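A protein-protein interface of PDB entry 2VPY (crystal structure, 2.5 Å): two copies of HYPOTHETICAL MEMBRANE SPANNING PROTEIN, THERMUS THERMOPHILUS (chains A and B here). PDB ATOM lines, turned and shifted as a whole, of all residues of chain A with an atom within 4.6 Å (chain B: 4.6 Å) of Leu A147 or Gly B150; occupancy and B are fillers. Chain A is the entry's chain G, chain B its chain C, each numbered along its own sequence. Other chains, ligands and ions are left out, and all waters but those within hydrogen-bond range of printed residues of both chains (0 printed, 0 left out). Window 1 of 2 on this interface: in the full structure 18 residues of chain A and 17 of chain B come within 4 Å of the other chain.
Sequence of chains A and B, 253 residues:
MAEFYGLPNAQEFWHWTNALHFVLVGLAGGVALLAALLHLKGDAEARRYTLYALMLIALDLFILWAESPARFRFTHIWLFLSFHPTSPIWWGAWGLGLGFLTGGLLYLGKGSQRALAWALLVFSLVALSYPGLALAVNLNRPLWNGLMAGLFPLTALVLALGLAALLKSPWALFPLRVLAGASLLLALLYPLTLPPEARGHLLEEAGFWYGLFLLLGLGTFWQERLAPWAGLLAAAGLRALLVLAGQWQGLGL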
ATOM      1  N   ASN A 145     -10.003 -13.014 -18.525  1.00  0.00           N
ATOM      2  CA  ASN A 145      -8.895 -12.061 -18.618  1.00  0.00           C
ATOM      3  C   ASN A 145      -9.248 -10.735 -19.298  1.00  0.00           C
ATOM      4  O   ASN A 145     -10.424 -10.427 -19.546  1.00  0.00           O
ATOM      5  CB  ASN A 145      -7.648 -12.680 -19.293  1.00  0.00           C
ATOM      6  CG  ASN A 145      -7.843 -13.012 -20.770  1.00  0.00           C
ATOM      7  OD1 ASN A 145      -6.970 -13.621 -21.396  1.00  0.00           O
ATOM      8  ND2 ASN A 145      -8.981 -12.613 -21.330  1.00  0.00           N
ATOM      9  N   GLY A 146      -8.212  -9.948 -19.564  1.00  0.00           N
ATOM     10  CA  GLY A 146      -8.363  -8.654 -20.197  1.00  0.00           C
ATOM     11  C   GLY A 146      -9.139  -8.643 -21.509  1.00  0.00           C
ATOM     12  O   GLY A 146      -9.810  -7.658 -21.801  1.00  0.00           O
ATOM     13  N   LEU A 147      -9.059  -9.712 -22.305  1.00  0.00           N
ATOM     14  CA  LEU A 147      -9.789  -9.784 -23.587  1.00  0.00           C
ATOM     15  C   LEU A 147     -11.315  -9.672 -23.487  1.00  0.00           C
ATOM     16  O   LEU A 147     -11.970  -9.339 -24.475  1.00  0.00           O
ATOM     17  CB  LEU A 147      -9.467 -11.061 -24.384  1.00  0.00           C
ATOM     18  CG  LEU A 147      -8.692 -10.843 -25.695  1.00  0.00           C
ATOM     19  CD1 LEU A 147      -8.705 -12.152 -26.488  1.00  0.00           C
ATOM     20  CD2 LEU A 147      -9.290  -9.688 -26.539  1.00  0.00           C
ATOM     21  N   MET A 148     -11.883  -9.984 -22.323  1.00  0.00           N
ATOM     22  CA  MET A 148     -13.325  -9.859 -22.103  1.00  0.00           C
ATOM     23  C   MET A 148     -13.741  -8.410 -22.324  1.00  0.00           C
ATOM     24  O   MET A 148     -14.840  -8.134 -22.808  1.00  0.00           O
ATOM     25  CB  MET A 148     -13.703 -10.220 -20.668  1.00  0.00           C
ATOM     26  CG  MET A 148     -13.356 -11.631 -20.237  1.00  0.00           C
ATOM     27  SD  MET A 148     -14.099 -12.926 -21.300  1.00  0.00           S
ATOM     28  CE  MET A 148     -12.714 -13.415 -22.295  1.00  0.00           C
ATOM     29  N   ALA A 149     -12.880  -7.477 -21.954  1.00  0.00           N
ATOM     30  CA  ALA A 149     -13.231  -6.078 -22.107  1.00  0.00           C
ATOM     31  C   ALA A 149     -13.260  -5.678 -23.579  1.00  0.00           C
ATOM     32  O   ALA A 149     -13.769  -4.611 -23.942  1.00  0.00           O
ATOM     33  CB  ALA A 149     -12.274  -5.183 -21.299  1.00  0.00           C
ATOM     34  N   GLY A 150     -12.736  -6.558 -24.427  1.00  0.00           N
ATOM     35  CA  GLY A 150     -12.699  -6.328 -25.864  1.00  0.00           C
ATOM     36  C   GLY A 150     -13.686  -7.236 -26.581  1.00  0.00           C
ATOM     37  O   GLY A 150     -14.390  -6.810 -27.500  1.00  0.00           O
ATOM     38  N   LEU A 151     -13.752  -8.494 -26.159  1.00  0.00           N
ATOM     39  CA  LEU A 151     -14.690  -9.433 -26.750  1.00  0.00           C
ATOM     40  C   LEU A 151     -16.167  -9.080 -26.508  1.00  0.00           C
ATOM     41  O   LEU A 151     -17.006  -9.415 -27.335  1.00  0.00           O
ATOM     42  CB  LEU A 151     -14.414 -10.863 -26.267  1.00  0.00           C
ATOM     43  CG  LEU A 151     -13.450 -11.555 -27.220  1.00  0.00           C
ATOM     44  CD1 LEU A 151     -12.994 -12.913 -26.702  1.00  0.00           C
ATOM     45  CD2 LEU A 151     -14.143 -11.686 -28.565  1.00  0.00           C
ATOM     46  N   LEU A 186     -10.534 -12.209 -32.708  1.00  0.00           N
ATOM     47  CA  LEU A 186     -10.121 -12.104 -31.306  1.00  0.00           C
ATOM     48  C   LEU A 186     -10.600 -13.359 -30.571  1.00  0.00           C
ATOM     49  O   LEU A 186      -9.937 -13.825 -29.644  1.00  0.00           O
ATOM     50  CB  LEU A 186     -10.722 -10.880 -30.572  1.00  0.00           C
ATOM     51  CG  LEU A 186     -10.557  -9.456 -31.101  1.00  0.00           C
ATOM     52  CD1 LEU A 186     -10.747  -8.426 -29.972  1.00  0.00           C
ATOM     53  CD2 LEU A 186      -9.184  -9.335 -31.735  1.00  0.00           C
ATOM     54  N   TYR A 190      -8.164 -15.691 -28.264  1.00  0.00           N
ATOM     55  CA  TYR A 190      -8.443 -15.831 -26.836  1.00  0.00           C
ATOM     56  C   TYR A 190      -7.792 -17.090 -26.147  1.00  0.00           C
ATOM     57  O   TYR A 190      -7.022 -16.932 -25.189  1.00  0.00           O
ATOM     58  CB  TYR A 190      -9.963 -15.780 -26.606  1.00  0.00           C
ATOM     59  CG  TYR A 190     -10.331 -16.040 -25.183  1.00  0.00           C
ATOM     60  CD1 TYR A 190      -9.941 -15.168 -24.166  1.00  0.00           C
ATOM     61  CD2 TYR A 190     -11.019 -17.199 -24.839  1.00  0.00           C
ATOM     62  CE1 TYR A 190     -10.226 -15.448 -22.840  1.00  0.00           C
ATOM     63  CE2 TYR A 190     -11.310 -17.491 -23.522  1.00  0.00           C
ATOM     64  CZ  TYR A 190     -10.914 -16.618 -22.529  1.00  0.00           C
ATOM     65  OH  TYR A 190     -11.217 -16.946 -21.238  1.00  0.00           O
ATOM     66  N   GLY B 146      -4.229 -10.216 -21.870  1.00  0.00           N
ATOM     67  CA  GLY B 146      -5.037 -10.671 -22.988  1.00  0.00           C
ATOM     68  C   GLY B 146      -5.513  -9.633 -24.007  1.00  0.00           C
ATOM     69  O   GLY B 146      -5.535  -9.933 -25.195  1.00  0.00           O
ATOM     70  N   LEU B 147      -5.874  -8.430 -23.554  1.00  0.00           N
ATOM     71  CA  LEU B 147      -6.338  -7.355 -24.454  1.00  0.00           C
ATOM     72  C   LEU B 147      -5.336  -7.005 -25.582  1.00  0.00           C
ATOM     73  O   LEU B 147      -5.711  -6.420 -26.598  1.00  0.00           O
ATOM     74  CB  LEU B 147      -6.685  -6.065 -23.686  1.00  0.00           C
ATOM     75  CG  LEU B 147      -8.102  -5.477 -23.587  1.00  0.00           C
ATOM     76  CD1 LEU B 147      -8.028  -4.016 -23.091  1.00  0.00           C
ATOM     77  CD2 LEU B 147      -8.826  -5.530 -24.945  1.00  0.00           C
ATOM     78  N   MET B 148      -4.058  -7.322 -25.357  1.00  0.00           N
ATOM     79  CA  MET B 148      -3.001  -7.043 -26.325  1.00  0.00           C
ATOM     80  C   MET B 148      -3.298  -7.842 -27.593  1.00  0.00           C
ATOM     81  O   MET B 148      -2.912  -7.448 -28.708  1.00  0.00           O
ATOM     82  CB  MET B 148      -1.622  -7.438 -25.787  1.00  0.00           C
ATOM     83  CG  MET B 148      -1.178  -6.668 -24.550  1.00  0.00           C
ATOM     84  SD  MET B 148      -1.034  -4.894 -24.842  1.00  0.00           S
ATOM     85  CE  MET B 148      -2.339  -4.272 -23.738  1.00  0.00           C
ATOM     86  N   ALA B 149      -3.957  -8.986 -27.419  1.00  0.00           N
ATOM     87  CA  ALA B 149      -4.327  -9.815 -28.554  1.00  0.00           C
ATOM     88  C   ALA B 149      -5.553  -9.172 -29.258  1.00  0.00           C
ATOM     89  O   ALA B 149      -5.915  -9.573 -30.361  1.00  0.00           O
ATOM     90  CB  ALA B 149      -4.652 -11.253 -28.106  1.00  0.00           C
ATOM     91  N   GLY B 150      -6.173  -8.186 -28.613  1.00  0.00           N
ATOM     92  CA  GLY B 150      -7.303  -7.500 -29.210  1.00  0.00           C
ATOM     93  C   GLY B 150      -6.903  -6.127 -29.728  1.00  0.00           C
ATOM     94  O   GLY B 150      -7.299  -5.694 -30.821  1.00  0.00           O
ATOM     95  N   LEU B 151      -6.098  -5.424 -28.940  1.00  0.00           N
ATOM     96  CA  LEU B 151      -5.604  -4.102 -29.284  1.00  0.00           C
ATOM     97  C   LEU B 151      -4.655  -4.120 -30.475  1.00  0.00           C
ATOM     98  O   LEU B 151      -4.684  -3.221 -31.314  1.00  0.00           O
ATOM     99  CB  LEU B 151      -4.890  -3.459 -28.079  1.00  0.00           C
ATOM    100  CG  LEU B 151      -5.824  -2.922 -26.984  1.00  0.00           C
ATOM    101  CD1 LEU B 151      -5.017  -2.347 -25.822  1.00  0.00           C
ATOM    102  CD2 LEU B 151      -6.748  -1.861 -27.590  1.00  0.00           C
ATOM    103  N   PHE B 152      -3.825  -5.147 -30.603  1.00  0.00           N
ATOM    104  CA  PHE B 152      -2.923  -5.095 -31.727  1.00  0.00           C
ATOM    105  C   PHE B 152      -3.558  -5.349 -33.112  1.00  0.00           C
ATOM    106  O   PHE B 152      -3.244  -4.621 -34.057  1.00  0.00           O
ATOM    107  CB  PHE B 152      -1.611  -5.827 -31.400  1.00  0.00           C
ATOM    108  CG  PHE B 152      -0.638  -4.985 -30.590  1.00  0.00           C
ATOM    109  CD1 PHE B 152      -0.948  -4.606 -29.285  1.00  0.00           C
ATOM    110  CD2 PHE B 152       0.544  -4.501 -31.166  1.00  0.00           C
ATOM    111  CE1 PHE B 152      -0.104  -3.759 -28.553  1.00  0.00           C
ATOM    112  CE2 PHE B 152       1.404  -3.646 -30.443  1.00  0.00           C
ATOM    113  CZ  PHE B 152       1.075  -3.275 -29.132  1.00  0.00           C
ATOM    114  N   PRO B 153      -4.463  -6.345 -33.247  1.00  0.00           N
ATOM    115  CA  PRO B 153      -5.105  -6.564 -34.553  1.00  0.00           C
ATOM    116  C   PRO B 153      -5.985  -5.349 -35.011  1.00  0.00           C
ATOM    117  O   PRO B 153      -5.941  -4.928 -36.168  1.00  0.00           O
ATOM    118  CB  PRO B 153      -5.945  -7.811 -34.333  1.00  0.00           C
ATOM    119  CG  PRO B 153      -5.119  -8.620 -33.389  1.00  0.00           C
ATOM    120  CD  PRO B 153      -4.487  -7.580 -32.439  1.00  0.00           C
ATOM    121  N   LEU B 154      -6.795  -4.796 -34.110  1.00  0.00           N
ATOM    122  CA  LEU B 154      -7.654  -3.657 -34.441  1.00  0.00           C
ATOM    123  C   LEU B 154      -6.859  -2.401 -34.781  1.00  0.00           C
ATOM    124  O   LEU B 154      -7.275  -1.582 -35.601  1.00  0.00           O
ATOM    125  CB  LEU B 154      -8.614  -3.324 -33.285  1.00  0.00           C
ATOM    126  CG  LEU B 154      -9.847  -4.228 -33.123  1.00  0.00           C
ATOM    127  CD1 LEU B 154     -10.365  -4.166 -31.678  1.00  0.00           C
ATOM    128  CD2 LEU B 154     -10.938  -3.819 -34.118  1.00  0.00           C
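Gly A146 touches Leu B147, and with the chains exchanged Leu A147 touches Gly B146.
Leu A147 touches its own counterpart, Leu B147.
Leu A147 touches Gly B150, but with the chains exchanged Gly A150 does not touch Leu B147 (4.1 Å).
Among the printed residues, merely in contact across the chains: Gly A146 with Leu B147 (3.3 Å), Leu A147 with Gly B146 (3.3 Å), Leu A186 with Ala B149 (3.6 Å), Leu A186 with Gly B150 (3.6 Å), Leu A147 with Leu B147 (3.7 Å), Asn A145 with Gly B146 (3.9 Å) and Leu A147 with Gly B150 (3.98 Å).
ND2 of Asn A145 lies close to N of Leu A147, 3.1 Å away.
Of the printed residues of chain B, Leu A147 touches Gly B146 (3.3 Å), Leu B147 (3.7 Å) and Gly B150 (3.98 Å).
Printed residues of chain A within 4 Å of Gly B150: Leu A147 (3.98 Å) and Leu A186 (3.6 Å).
Printed residues of chain A within 4 Å of Leu B147: Gly A146 (3.3 Å) and Leu A147 (3.7 Å).
Printed residues of chain A within 4 Å of Ala B149: Leu A186.
Printed residues of chain B within 4 Å of Leu A186: Ala B149 and Gly B150.
Leu B151 touches none of the printed residues of chain A.
Phe B152 touches none of the printed residues of chain A.
The nearest printed residue of chain A that does not touch Gly B150 is Gly A150 (6.5 Å).
Of the 9 printed residues of chain A, 4 touch a printed residue of chain B.
Hydrophobic or aromatic side chains of chain A that line the printed part of chain B: Leu A147 and Leu A186.
Among the printed residues, 7 pairs touch across the chains.
Among the printed residues, no Asp or Glu carboxylate lies within 4 Å of a Lys or Arg side-chain nitrogen of the other chain.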
